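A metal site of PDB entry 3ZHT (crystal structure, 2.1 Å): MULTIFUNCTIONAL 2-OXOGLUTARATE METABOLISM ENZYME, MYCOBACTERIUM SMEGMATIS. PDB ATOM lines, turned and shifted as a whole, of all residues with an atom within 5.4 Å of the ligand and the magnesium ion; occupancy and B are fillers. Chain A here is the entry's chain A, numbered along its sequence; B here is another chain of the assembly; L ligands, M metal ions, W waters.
N1 of the ligand lies close to OE1 of Gln 617 of chain B (3.4 Å).
Merely in contact with the ligand: Arg 146 (3.999 Å), His 246 (3.5 Å), Gly 285 (3.4 Å), Gln 292 (3.7 Å), Gly 322 (3.5 Å), Phe 323 (3.4 Å), Gln 542 of chain B (3.2 Å), Leu 591 of chain B (3.5 Å), Phe 618 of chain B (3.6 Å) and Phe 621 of chain B (3.3 Å).
The nearest printed residue that does not touch the ligand is Thr 548 of chain B (4.1 Å).
Water W3 lies within hydrogen-bond range of O of Val 317 (2.5 Å), N of Asp 286 (3.1 Å), O7 of the ligand (3.2 Å) and ND2 of Asn 319 (3.5 Å).
Water W2 lies within hydrogen-bond range of an oxygen (O4) of the ligand (2.7 Å) and the backbone NH of Gly 285 (3.4 Å).
Water W4 lies within hydrogen-bond range of ND1 of His 388, NH1 of Arg 384, N of Phe 323 and O9 of the ligand.
OE1 of Glu 593 of chain B lies within hydrogen-bond range of NE2 of Gln 292, 3.1 Å away.
The guanidinium group (NH2) of Arg 181 sits at hydrogen-bond distance from a ring nitrogen (ND1) of His 388 (3.4 Å).
O of Gln 542 of chain B lies within hydrogen-bond range of NE2 of Gln 617 of chain B.
OG1 of Thr 548 of chain B sits at hydrogen-bond distance from NE2 of Gln 617 of chain B, at 2.8 Å.
The side-chain carboxylate (OD2) of Asp 543 of chain B sits at hydrogen-bond distance from the side-chain amide nitrogen (NE2) of Gln 617 of chain B (3.0 Å).
The backbone carbonyl oxygen of Phe 323 lies within hydrogen-bond range of the guanidinium group of Arg 384 (2.9 Å).
O of Leu 591 of chain B sits at hydrogen-bond distance from NE2 of Gln 292.
O of Arg 146 sits close to NE2 of His 180 (3.4 Å).
The magnesium ion is bound by O of Ile 321 (2.0 Å), O5 of the ligand (2.1 Å), OD1 of Asp 286 (2.1 Å), O6 of the ligand (2.2 Å), water W3 (2.2 Å) and OD1 of Asn 319 (2.2 Å).
The magnesium ion has six donor atoms within binding distance.
N2 of the ligand lies within hydrogen-bond range of OE2 of Glu 593 of chain B (2.7 Å).
N4 of the ligand sits at hydrogen-bond distance from O of Ser 245.
O7 of the ligand lies within salt-bridge range of NE of Arg 181 (2.8 Å).
N of Ala 287 is in hydrogen-bond range of O4 of the ligand (3.5 Å).
N of Ala 288 lies within hydrogen-bond range of O4 of the ligand.
ND2 of Asn 389 lies within hydrogen-bond range of O2 of the ligand.
The backbone NH (N) of Leu 247 is in hydrogen-bond range of a nitrogen (N3) of the ligand.
A ring nitrogen (NE2) of His 661 of chain B is in hydrogen-bond range of an oxygen (O1) of the ligand (3.1 Å).
A ring nitrogen (NE2) of His 388 sits close to a sulfur (S1) of the ligand (3.3 Å).
Within 4 Å of the magnesium ion: Asp 286, Asn 319 and Ile 321.
The nearest printed residue that does not touch the magnesium ion is Gly 322 (4.1 Å).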
ATOM      1  N   ARG A 146      -7.006  -4.042   6.538  1.00  0.00           N
ATOM      2  CA  ARG A 146      -6.233  -4.483   7.726  1.00  0.00           C
ATOM      3  C   ARG A 146      -5.549  -5.865   7.555  1.00  0.00           C
ATOM      4  O   ARG A 146      -4.658  -6.211   8.335  1.00  0.00           O
ATOM      5  CB  ARG A 146      -7.085  -4.451   9.028  1.00  0.00           C
ATOM      6  CG  ARG A 146      -7.974  -5.659   9.353  1.00  0.00           C
ATOM      7  CD  ARG A 146      -8.763  -5.428  10.641  1.00  0.00           C
ATOM      8  NE  ARG A 146      -9.965  -6.264  10.693  1.00  0.00           N
ATOM      9  CZ  ARG A 146     -10.534  -6.725  11.810  1.00  0.00           C
ATOM     10  NH1 ARG A 146     -10.031  -6.417  12.998  1.00  0.00           N
ATOM     11  NH2 ARG A 146     -11.614  -7.500  11.740  1.00  0.00           N
ATOM     12  N   HIS A 180      -2.873 -12.006  11.838  1.00  0.00           N
ATOM     13  CA  HIS A 180      -3.832 -12.000  10.730  1.00  0.00           C
ATOM     14  C   HIS A 180      -3.316 -11.475   9.370  1.00  0.00           C
ATOM     15  O   HIS A 180      -3.913 -11.833   8.363  1.00  0.00           O
ATOM     16  CB  HIS A 180      -5.097 -11.220  11.125  1.00  0.00           C
ATOM     17  CG  HIS A 180      -4.850  -9.780  11.459  1.00  0.00           C
ATOM     18  ND1 HIS A 180      -4.900  -9.332  12.773  1.00  0.00           N
ATOM     19  CD2 HIS A 180      -4.561  -8.737  10.648  1.00  0.00           C
ATOM     20  CE1 HIS A 180      -4.642  -8.036  12.719  1.00  0.00           C
ATOM     21  NE2 HIS A 180      -4.404  -7.629  11.464  1.00  0.00           N
ATOM     22  N   ARG A 181      -2.264 -10.626   9.334  1.00  0.00           N
ATOM     23  CA  ARG A 181      -1.734 -10.010   8.119  1.00  0.00           C
ATOM     24  C   ARG A 181      -1.164 -11.070   7.103  1.00  0.00           C
ATOM     25  O   ARG A 181      -0.160 -11.721   7.363  1.00  0.00           O
ATOM     26  CB  ARG A 181      -0.662  -8.941   8.456  1.00  0.00           C
ATOM     27  CG  ARG A 181      -0.283  -8.063   7.256  1.00  0.00           C
ATOM     28  CD  ARG A 181       0.647  -6.889   7.590  1.00  0.00           C
ATOM     29  NE  ARG A 181       0.078  -6.013   8.623  1.00  0.00           N
ATOM     30  CZ  ARG A 181      -0.841  -5.079   8.397  1.00  0.00           C
ATOM     31  NH1 ARG A 181      -1.308  -4.873   7.175  1.00  0.00           N
ATOM     32  NH2 ARG A 181      -1.304  -4.339   9.405  1.00  0.00           N
ATOM     33  N   SER A 245      -7.017 -12.579  18.467  1.00  0.00           N
ATOM     34  CA  SER A 245      -6.407 -11.358  17.934  1.00  0.00           C
ATOM     35  C   SER A 245      -5.185 -10.954  18.776  1.00  0.00           C
ATOM     36  O   SER A 245      -4.330 -10.220  18.276  1.00  0.00           O
ATOM     37  CB  SER A 245      -7.396 -10.212  17.910  1.00  0.00           C
ATOM     38  OG  SER A 245      -8.474 -10.473  17.043  1.00  0.00           O
ATOM     39  N   HIS A 246      -5.111 -11.424  20.059  1.00  0.00           N
ATOM     40  CA  HIS A 246      -4.027 -11.157  21.004  1.00  0.00           C
ATOM     41  C   HIS A 246      -2.734 -11.601  20.408  1.00  0.00           C
ATOM     42  O   HIS A 246      -2.440 -12.791  20.372  1.00  0.00           O
ATOM     43  CB  HIS A 246      -4.269 -11.859  22.361  1.00  0.00           C
ATOM     44  CG  HIS A 246      -5.434 -11.292  23.095  1.00  0.00           C
ATOM     45  ND1 HIS A 246      -6.690 -11.253  22.531  1.00  0.00           N
ATOM     46  CD2 HIS A 246      -5.501 -10.802  24.355  1.00  0.00           C
ATOM     47  CE1 HIS A 246      -7.479 -10.709  23.446  1.00  0.00           C
ATOM     48  NE2 HIS A 246      -6.809 -10.434  24.556  1.00  0.00           N
ATOM     49  N   LEU A 247      -1.999 -10.643  19.858  1.00  0.00           N
ATOM     50  CA  LEU A 247      -0.758 -10.899  19.154  1.00  0.00           C
ATOM     51  C   LEU A 247       0.256 -11.609  20.058  1.00  0.00           C
ATOM     52  O   LEU A 247       0.402 -11.279  21.237  1.00  0.00           O
ATOM     53  CB  LEU A 247      -0.169  -9.569  18.613  1.00  0.00           C
ATOM     54  CG  LEU A 247      -1.060  -8.833  17.591  1.00  0.00           C
ATOM     55  CD1 LEU A 247      -0.668  -7.377  17.424  1.00  0.00           C
ATOM     56  CD2 LEU A 247      -1.115  -9.573  16.286  1.00  0.00           C
ATOM     57  N   GLY A 285       4.859  -9.717  13.943  1.00  0.00           N
ATOM     58  CA  GLY A 285       4.875  -8.318  13.516  1.00  0.00           C
ATOM     59  C   GLY A 285       5.986  -7.667  14.306  1.00  0.00           C
ATOM     60  O   GLY A 285       6.343  -8.168  15.393  1.00  0.00           O
ATOM     61  N   ASP A 286       6.576  -6.602  13.780  1.00  0.00           N
ATOM     62  CA  ASP A 286       7.705  -5.952  14.444  1.00  0.00           C
ATOM     63  C   ASP A 286       7.330  -5.327  15.799  1.00  0.00           C
ATOM     64  O   ASP A 286       8.135  -5.452  16.730  1.00  0.00           O
ATOM     65  CB  ASP A 286       8.370  -4.902  13.534  1.00  0.00           C
ATOM     66  CG  ASP A 286       7.468  -3.795  13.001  1.00  0.00           C
ATOM     67  OD1 ASP A 286       6.473  -4.125  12.308  1.00  0.00           O
ATOM     68  OD2 ASP A 286       7.750  -2.612  13.275  1.00  0.00           O
ATOM     69  N   ALA A 287       6.148  -4.642  15.907  1.00  0.00           N
ATOM     70  CA  ALA A 287       5.831  -3.991  17.187  1.00  0.00           C
ATOM     71  C   ALA A 287       5.524  -5.024  18.274  1.00  0.00           C
ATOM     72  O   ALA A 287       6.061  -4.906  19.368  1.00  0.00           O
ATOM     73  CB  ALA A 287       4.686  -2.963  17.029  1.00  0.00           C
ATOM     74  N   ALA A 288       4.776  -6.089  17.927  1.00  0.00           N
ATOM     75  CA  ALA A 288       4.360  -7.152  18.850  1.00  0.00           C
ATOM     76  C   ALA A 288       5.549  -7.991  19.349  1.00  0.00           C
ATOM     77  O   ALA A 288       5.614  -8.346  20.532  1.00  0.00           O
ATOM     78  CB  ALA A 288       3.340  -8.043  18.166  1.00  0.00           C
ATOM     79  N   PHE A 289       6.491  -8.339  18.428  1.00  0.00           N
ATOM     80  CA  PHE A 289       7.667  -9.153  18.767  1.00  0.00           C
ATOM     81  C   PHE A 289       8.504  -8.471  19.839  1.00  0.00           C
ATOM     82  O   PHE A 289       9.023  -9.141  20.722  1.00  0.00           O
ATOM     83  CB  PHE A 289       8.516  -9.462  17.489  1.00  0.00           C
ATOM     84  CG  PHE A 289       9.495 -10.605  17.675  1.00  0.00           C
ATOM     85  CD1 PHE A 289       9.040 -11.912  17.842  1.00  0.00           C
ATOM     86  CD2 PHE A 289      10.862 -10.384  17.701  1.00  0.00           C
ATOM     87  CE1 PHE A 289       9.942 -12.966  17.996  1.00  0.00           C
ATOM     88  CE2 PHE A 289      11.767 -11.444  17.862  1.00  0.00           C
ATOM     89  CZ  PHE A 289      11.297 -12.730  17.998  1.00  0.00           C
ATOM     90  N   GLN A 292       5.616  -7.731  23.531  1.00  0.00           N
ATOM     91  CA  GLN A 292       4.903  -8.776  24.259  1.00  0.00           C
ATOM     92  C   GLN A 292       5.856  -9.664  25.033  1.00  0.00           C
ATOM     93  O   GLN A 292       6.722 -10.291  24.427  1.00  0.00           O
ATOM     94  CB  GLN A 292       4.044  -9.599  23.271  1.00  0.00           C
ATOM     95  CG  GLN A 292       2.821  -8.846  22.718  1.00  0.00           C
ATOM     96  CD  GLN A 292       1.826  -8.535  23.822  1.00  0.00           C
ATOM     97  OE1 GLN A 292       1.300  -9.427  24.485  1.00  0.00           O
ATOM     98  NE2 GLN A 292       1.572  -7.260  24.091  1.00  0.00           N
ATOM     99  N   VAL A 317       7.643  -9.986  10.138  1.00  0.00           N
ATOM    100  CA  VAL A 317       7.237  -9.170   9.014  1.00  0.00           C
ATOM    101  C   VAL A 317       7.407  -7.735   9.499  1.00  0.00           C
ATOM    102  O   VAL A 317       6.487  -7.135  10.074  1.00  0.00           O
ATOM    103  CB  VAL A 317       5.814  -9.509   8.508  1.00  0.00           C
ATOM    104  CG1 VAL A 317       5.468  -8.669   7.267  1.00  0.00           C
ATOM    105  CG2 VAL A 317       5.686 -10.990   8.192  1.00  0.00           C
ATOM    106  N   ASN A 319       7.506  -4.331   8.971  1.00  0.00           N
ATOM    107  CA  ASN A 319       7.049  -3.278   8.071  1.00  0.00           C
ATOM    108  C   ASN A 319       7.296  -1.885   8.685  1.00  0.00           C
ATOM    109  O   ASN A 319       6.765  -0.871   8.222  1.00  0.00           O
ATOM    110  CB  ASN A 319       5.588  -3.490   7.668  1.00  0.00           C
ATOM    111  CG  ASN A 319       4.632  -3.644   8.815  1.00  0.00           C
ATOM    112  OD1 ASN A 319       4.915  -3.243   9.937  1.00  0.00           O
ATOM    113  ND2 ASN A 319       3.453  -4.180   8.539  1.00  0.00           N
ATOM    114  N   GLN A 320       8.155  -1.856   9.747  1.00  0.00           N
ATOM    115  CA  GLN A 320       8.717  -0.679  10.427  1.00  0.00           C
ATOM    116  C   GLN A 320       7.637   0.265  10.948  1.00  0.00           C
ATOM    117  O   GLN A 320       7.805   1.480  10.934  1.00  0.00           O
ATOM    118  CB  GLN A 320       9.690   0.054   9.468  1.00  0.00           C
ATOM    119  CG  GLN A 320      10.727  -0.894   8.824  1.00  0.00           C
ATOM    120  CD  GLN A 320      11.653  -0.198   7.849  1.00  0.00           C
ATOM    121  OE1 GLN A 320      12.550   0.555   8.225  1.00  0.00           O
ATOM    122  NE2 GLN A 320      11.475  -0.466   6.571  1.00  0.00           N
ATOM    123  N   ILE A 321       6.522  -0.324  11.397  1.00  0.00           N
ATOM    124  CA  ILE A 321       5.371   0.417  11.930  1.00  0.00           C
ATOM    125  C   ILE A 321       4.471  -0.534  12.695  1.00  0.00           C
ATOM    126  O   ILE A 321       4.426  -1.746  12.391  1.00  0.00           O
ATOM    127  CB  ILE A 321       4.600   1.167  10.781  1.00  0.00           C
ATOM    128  CG1 ILE A 321       3.694   2.293  11.340  1.00  0.00           C
ATOM    129  CG2 ILE A 321       3.882   0.208   9.777  1.00  0.00           C
ATOM    130  CD1 ILE A 321       3.294   3.324  10.333  1.00  0.00           C
ATOM    131  N   GLY A 322       3.749   0.037  13.635  1.00  0.00           N
ATOM    132  CA  GLY A 322       2.781  -0.663  14.471  1.00  0.00           C
ATOM    133  C   GLY A 322       1.555   0.211  14.572  1.00  0.00           C
ATOM    134  O   GLY A 322       1.478   1.077  15.454  1.00  0.00           O
ATOM    135  N   PHE A 323       0.620   0.047  13.612  1.00  0.00           N
ATOM    136  CA  PHE A 323      -0.592   0.817  13.428  1.00  0.00           C
ATOM    137  C   PHE A 323      -0.163   2.281  13.094  1.00  0.00           C
ATOM    138  O   PHE A 323       0.186   2.554  11.955  1.00  0.00           O
ATOM    139  CB  PHE A 323      -1.555   0.685  14.659  1.00  0.00           C
ATOM    140  CG  PHE A 323      -2.977   1.153  14.476  1.00  0.00           C
ATOM    141  CD1 PHE A 323      -3.310   2.097  13.507  1.00  0.00           C
ATOM    142  CD2 PHE A 323      -3.988   0.659  15.290  1.00  0.00           C
ATOM    143  CE1 PHE A 323      -4.619   2.548  13.362  1.00  0.00           C
ATOM    144  CE2 PHE A 323      -5.305   1.104  15.145  1.00  0.00           C
ATOM    145  CZ  PHE A 323      -5.617   2.036  14.172  1.00  0.00           C
ATOM    146  N   ARG A 384       4.357  -1.351   4.846  1.00  0.00           N
ATOM    147  CA  ARG A 384       2.925  -1.535   4.799  1.00  0.00           C
ATOM    148  C   ARG A 384       2.472  -0.500   3.794  1.00  0.00           C
ATOM    149  O   ARG A 384       2.562   0.688   4.060  1.00  0.00           O
ATOM    150  CB  ARG A 384       2.349  -1.342   6.220  1.00  0.00           C
ATOM    151  CG  ARG A 384       0.944  -1.886   6.423  1.00  0.00           C
ATOM    152  CD  ARG A 384       0.350  -1.247   7.646  1.00  0.00           C
ATOM    153  NE  ARG A 384       0.131   0.185   7.433  1.00  0.00           N
ATOM    154  CZ  ARG A 384       0.084   1.092   8.393  1.00  0.00           C
ATOM    155  NH1 ARG A 384       0.207   0.739   9.667  1.00  0.00           N
ATOM    156  NH2 ARG A 384      -0.130   2.374   8.089  1.00  0.00           N
ATOM    157  N   HIS A 388      -3.340   1.045   7.966  1.00  0.00           N
ATOM    158  CA  HIS A 388      -3.555  -0.083   8.866  1.00  0.00           C
ATOM    159  C   HIS A 388      -4.986  -0.657   8.686  1.00  0.00           C
ATOM    160  O   HIS A 388      -5.123  -1.875   8.617  1.00  0.00           O
ATOM    161  CB  HIS A 388      -3.304   0.343  10.333  1.00  0.00           C
ATOM    162  CG  HIS A 388      -3.183  -0.799  11.282  1.00  0.00           C
ATOM    163  ND1 HIS A 388      -2.057  -1.630  11.285  1.00  0.00           N
ATOM    164  CD2 HIS A 388      -4.060  -1.260  12.198  1.00  0.00           C
ATOM    165  CE1 HIS A 388      -2.273  -2.529  12.236  1.00  0.00           C
ATOM    166  NE2 HIS A 388      -3.475  -2.367  12.805  1.00  0.00           N
ATOM    167  N   ASN A 389      -6.027   0.215   8.567  1.00  0.00           N
ATOM    168  CA  ASN A 389      -7.440  -0.167   8.376  1.00  0.00           C
ATOM    169  C   ASN A 389      -8.211   0.929   7.591  1.00  0.00           C
ATOM    170  O   ASN A 389      -7.614   1.944   7.211  1.00  0.00           O
ATOM    171  CB  ASN A 389      -8.134  -0.491   9.725  1.00  0.00           C
ATOM    172  CG  ASN A 389      -8.182   0.611  10.752  1.00  0.00           C
ATOM    173  OD1 ASN A 389      -8.120   1.811  10.468  1.00  0.00           O
ATOM    174  ND2 ASN A 389      -8.418   0.219  11.978  1.00  0.00           N
ATOM    175  N   GLN B 542      -1.876   2.360  23.347  1.00  0.00           N
ATOM    176  CA  GLN B 542      -1.510   2.046  21.959  1.00  0.00           C
ATOM    177  C   GLN B 542      -2.203   3.000  20.975  1.00  0.00           C
ATOM    178  O   GLN B 542      -3.437   3.067  20.951  1.00  0.00           O
ATOM    179  CB  GLN B 542      -1.799   0.577  21.651  1.00  0.00           C
ATOM    180  CG  GLN B 542      -0.787  -0.350  22.318  1.00  0.00           C
ATOM    181  CD  GLN B 542      -1.362  -1.705  22.628  1.00  0.00           C
ATOM    182  OE1 GLN B 542      -2.303  -2.174  21.997  1.00  0.00           O
ATOM    183  NE2 GLN B 542      -0.799  -2.373  23.620  1.00  0.00           N
ATOM    184  N   ASP B 543      -1.380   3.818  20.262  1.00  0.00           N
ATOM    185  CA  ASP B 543      -1.808   4.819  19.261  1.00  0.00           C
ATOM    186  C   ASP B 543      -2.731   5.884  19.865  1.00  0.00           C
ATOM    187  O   ASP B 543      -3.594   6.420  19.161  1.00  0.00           O
ATOM    188  CB  ASP B 543      -2.504   4.139  18.058  1.00  0.00           C
ATOM    189  CG  ASP B 543      -1.690   3.036  17.455  1.00  0.00           C
ATOM    190  OD1 ASP B 543      -0.699   3.354  16.791  1.00  0.00           O
ATOM    191  OD2 ASP B 543      -1.964   1.848  17.771  1.00  0.00           O
ATOM    192  N   THR B 548      -7.143   5.270  18.361  1.00  0.00           N
ATOM    193  CA  THR B 548      -7.404   4.030  17.623  1.00  0.00           C
ATOM    194  C   THR B 548      -8.505   4.237  16.564  1.00  0.00           C
ATOM    195  O   THR B 548      -8.404   3.694  15.474  1.00  0.00           O
ATOM    196  CB  THR B 548      -7.793   2.944  18.635  1.00  0.00           C
ATOM    197  OG1 THR B 548      -6.669   2.685  19.479  1.00  0.00           O
ATOM    198  CG2 THR B 548      -8.298   1.626  17.974  1.00  0.00           C
ATOM    199  N   PHE B 549      -9.521   5.056  16.891  1.00  0.00           N
ATOM    200  CA  PHE B 549     -10.646   5.301  16.012  1.00  0.00           C
ATOM    201  C   PHE B 549     -10.526   6.658  15.326  1.00  0.00           C
ATOM    202  O   PHE B 549     -11.517   7.187  14.847  1.00  0.00           O
ATOM    203  CB  PHE B 549     -11.983   5.153  16.788  1.00  0.00           C
ATOM    204  CG  PHE B 549     -11.989   3.901  17.634  1.00  0.00           C
ATOM    205  CD1 PHE B 549     -12.317   2.676  17.082  1.00  0.00           C
ATOM    206  CD2 PHE B 549     -11.599   3.937  18.978  1.00  0.00           C
ATOM    207  CE1 PHE B 549     -12.246   1.509  17.844  1.00  0.00           C
ATOM    208  CE2 PHE B 549     -11.535   2.764  19.739  1.00  0.00           C
ATOM    209  CZ  PHE B 549     -11.867   1.561  19.164  1.00  0.00           C
ATOM    210  N   LEU B 591       3.890  -1.909  22.383  1.00  0.00           N
ATOM    211  CA  LEU B 591       2.818  -2.873  22.247  1.00  0.00           C
ATOM    212  C   LEU B 591       2.850  -3.812  23.454  1.00  0.00           C
ATOM    213  O   LEU B 591       3.195  -4.982  23.343  1.00  0.00           O
ATOM    214  CB  LEU B 591       2.914  -3.627  20.912  1.00  0.00           C
ATOM    215  CG  LEU B 591       1.584  -4.067  20.306  1.00  0.00           C
ATOM    216  CD1 LEU B 591       1.734  -4.308  18.811  1.00  0.00           C
ATOM    217  CD2 LEU B 591       0.995  -5.306  21.012  1.00  0.00           C
ATOM    218  N   GLU B 593       0.760  -4.558  27.423  1.00  0.00           N
ATOM    219  CA  GLU B 593      -0.357  -4.275  28.319  1.00  0.00           C
ATOM    220  C   GLU B 593       0.135  -4.392  29.744  1.00  0.00           C
ATOM    221  O   GLU B 593      -0.046  -3.467  30.508  1.00  0.00           O
ATOM    222  CB  GLU B 593      -1.561  -5.192  28.070  1.00  0.00           C
ATOM    223  CG  GLU B 593      -2.327  -4.807  26.814  1.00  0.00           C
ATOM    224  CD  GLU B 593      -1.782  -5.342  25.503  1.00  0.00           C
ATOM    225  OE1 GLU B 593      -1.072  -6.371  25.519  1.00  0.00           O
ATOM    226  OE2 GLU B 593      -2.081  -4.738  24.457  1.00  0.00           O
ATOM    227  N   GLN B 617      -6.163  -0.454  23.480  1.00  0.00           N
ATOM    228  CA  GLN B 617      -6.514  -0.308  22.072  1.00  0.00           C
ATOM    229  C   GLN B 617      -8.010  -0.633  21.921  1.00  0.00           C
ATOM    230  O   GLN B 617      -8.760   0.128  21.328  1.00  0.00           O
ATOM    231  CB  GLN B 617      -5.620  -1.205  21.179  1.00  0.00           C
ATOM    232  CG  GLN B 617      -5.886  -0.968  19.687  1.00  0.00           C
ATOM    233  CD  GLN B 617      -4.707  -0.370  18.980  1.00  0.00           C
ATOM    234  OE1 GLN B 617      -3.908  -1.073  18.381  1.00  0.00           O
ATOM    235  NE2 GLN B 617      -4.547   0.935  19.031  1.00  0.00           N
ATOM    236  N   PHE B 618      -8.392  -1.775  22.490  1.00  0.00           N
ATOM    237  CA  PHE B 618      -9.738  -2.346  22.685  1.00  0.00           C
ATOM    238  C   PHE B 618      -9.687  -2.907  24.100  1.00  0.00           C
ATOM    239  O   PHE B 618      -8.634  -3.429  24.462  1.00  0.00           O
ATOM    240  CB  PHE B 618     -10.049  -3.421  21.628  1.00  0.00           C
ATOM    241  CG  PHE B 618     -10.399  -2.867  20.261  1.00  0.00           C
ATOM    242  CD1 PHE B 618      -9.407  -2.507  19.353  1.00  0.00           C
ATOM    243  CD2 PHE B 618     -11.729  -2.738  19.870  1.00  0.00           C
ATOM    244  CE1 PHE B 618      -9.739  -1.998  18.089  1.00  0.00           C
ATOM    245  CE2 PHE B 618     -12.068  -2.235  18.606  1.00  0.00           C
ATOM    246  CZ  PHE B 618     -11.064  -1.861  17.727  1.00  0.00           C
ATOM    247  N   PHE B 621      -7.965  -6.484  25.260  1.00  0.00           N
ATOM    248  CA  PHE B 621      -6.542  -6.756  25.432  1.00  0.00           C
ATOM    249  C   PHE B 621      -6.036  -6.463  26.841  1.00  0.00           C
ATOM    250  O   PHE B 621      -4.889  -6.824  27.138  1.00  0.00           O
ATOM    251  CB  PHE B 621      -5.720  -5.969  24.386  1.00  0.00           C
ATOM    252  CG  PHE B 621      -6.151  -6.312  22.972  1.00  0.00           C
ATOM    253  CD1 PHE B 621      -6.020  -7.598  22.495  1.00  0.00           C
ATOM    254  CD2 PHE B 621      -6.718  -5.350  22.154  1.00  0.00           C
ATOM    255  CE1 PHE B 621      -6.498  -7.933  21.226  1.00  0.00           C
ATOM    256  CE2 PHE B 621      -7.188  -5.680  20.871  1.00  0.00           C
ATOM    257  CZ  PHE B 621      -7.066  -6.971  20.407  1.00  0.00           C
ATOM    258  N   GLN B 657     -17.466  -6.941  15.540  1.00  0.00           N
ATOM    259  CA  GLN B 657     -16.051  -7.047  15.204  1.00  0.00           C
ATOM    260  C   GLN B 657     -15.357  -8.264  15.841  1.00  0.00           C
ATOM    261  O   GLN B 657     -14.142  -8.367  15.759  1.00  0.00           O
ATOM    262  CB  GLN B 657     -15.303  -5.771  15.603  1.00  0.00           C
ATOM    263  CG  GLN B 657     -15.391  -4.636  14.606  1.00  0.00           C
ATOM    264  CD  GLN B 657     -14.227  -3.718  14.888  1.00  0.00           C
ATOM    265  OE1 GLN B 657     -14.171  -3.084  15.965  1.00  0.00           O
ATOM    266  NE2 GLN B 657     -13.175  -3.819  14.054  1.00  0.00           N
ATOM    267  N   HIS B 661     -12.669  -7.834  19.853  1.00  0.00           N
ATOM    268  CA  HIS B 661     -12.867  -6.424  19.551  1.00  0.00           C
ATOM    269  C   HIS B 661     -14.275  -6.020  20.019  1.00  0.00           C
ATOM    270  O   HIS B 661     -14.973  -5.257  19.337  1.00  0.00           O
ATOM    271  CB  HIS B 661     -12.663  -6.143  18.044  1.00  0.00           C
ATOM    272  CG  HIS B 661     -11.242  -6.335  17.622  1.00  0.00           C
ATOM    273  ND1 HIS B 661     -10.780  -7.562  17.182  1.00  0.00           N
ATOM    274  CD2 HIS B 661     -10.210  -5.464  17.675  1.00  0.00           C
ATOM    275  CE1 HIS B 661      -9.493  -7.389  16.941  1.00  0.00           C
ATOM    276  NE2 HIS B 661      -9.108  -6.144  17.220  1.00  0.00           N
HETATM  277  S1  LIG L   1      -2.880  -4.417  15.330  1.00  0.00           S
HETATM  278  C1  LIG L   1      -3.946  -4.761  16.558  1.00  0.00           C
HETATM  279  N1  LIG L   1      -3.448  -4.353  17.867  1.00  0.00           N
HETATM  280  C2  LIG L   1      -2.197  -3.742  17.704  1.00  0.00           C
HETATM  281  C3  LIG L   1      -1.772  -3.740  16.346  1.00  0.00           C
HETATM  282  C4  LIG L   1      -5.344  -5.357  16.281  1.00  0.00           C
HETATM  283  C5  LIG L   1      -6.285  -4.451  15.500  1.00  0.00           C
HETATM  284  O1  LIG L   1      -6.055  -5.976  17.347  1.00  0.00           O
HETATM  285  P1  LIG L   1       2.810  -5.086  14.522  1.00  0.00           P
HETATM  286  P2  LIG L   1       1.447  -5.086  11.813  1.00  0.00           P
HETATM  287  N2  LIG L   1      -2.318  -6.046  22.090  1.00  0.00           N
HETATM  288  C6  LIG L   1      -6.605  -3.125  16.173  1.00  0.00           C
HETATM  289  O2  LIG L   1      -8.748  -0.914  14.774  1.00  0.00           O
HETATM  290  C7  LIG L   1      -6.694  -1.973  15.176  1.00  0.00           C
HETATM  291  O3  LIG L   1      -8.256  -2.632  13.455  1.00  0.00           O
HETATM  292  C8  LIG L   1      -7.975  -1.890  14.380  1.00  0.00           C
HETATM  293  O4  LIG L   1       3.091  -6.206  15.462  1.00  0.00           O
HETATM  294  O5  LIG L   1       2.392  -3.904  11.508  1.00  0.00           O
HETATM  295  C9  LIG L   1      -2.361  -7.342  21.742  1.00  0.00           C
HETATM  296  C10 LIG L   1      -1.792  -8.329  22.711  1.00  0.00           C
HETATM  297  O6  LIG L   1       3.986  -4.199  14.089  1.00  0.00           O
HETATM  298  O7  LIG L   1       1.733  -6.273  10.874  1.00  0.00           O
HETATM  299  N3  LIG L   1      -2.928  -7.833  20.631  1.00  0.00           N
HETATM  300  C11 LIG L   1      -4.111  -4.487  19.186  1.00  0.00           C
HETATM  301  O8  LIG L   1       2.152  -5.415  13.174  1.00  0.00           O
HETATM  302  O9  LIG L   1       0.025  -4.698  11.940  1.00  0.00           O
HETATM  303  C12 LIG L   1      -3.540  -6.960  19.800  1.00  0.00           C
HETATM  304  N4  LIG L   1      -4.197  -7.484  18.762  1.00  0.00           N
HETATM  305  C13 LIG L   1      -1.499  -3.027  18.813  1.00  0.00           C
HETATM  306  C14 LIG L   1      -3.545  -5.566  20.082  1.00  0.00           C
HETATM  307  C15 LIG L   1      -0.463  -3.189  15.843  1.00  0.00           C
HETATM  308  C16 LIG L   1       0.397  -4.324  15.351  1.00  0.00           C
HETATM  309  O10 LIG L   1       1.769  -3.962  15.028  1.00  0.00           O
HETATM  310  C17 LIG L   1      -2.925  -5.197  21.254  1.00  0.00           C
HETATM  311 MG    MG M   1       4.410  -3.718  12.028  1.00  0.00          MG
HETATM  312  O   HOH W   1       1.479  -8.672  11.830  1.00  0.00           O
HETATM  313  O   HOH W   2       1.781  -8.480  14.763  1.00  0.00           O
HETATM  314  O   HOH W   3       4.880  -5.715  11.285  1.00  0.00           O
HETATM  315  O   HOH W   4       0.589  -1.741  11.133  1.00  0.00           O
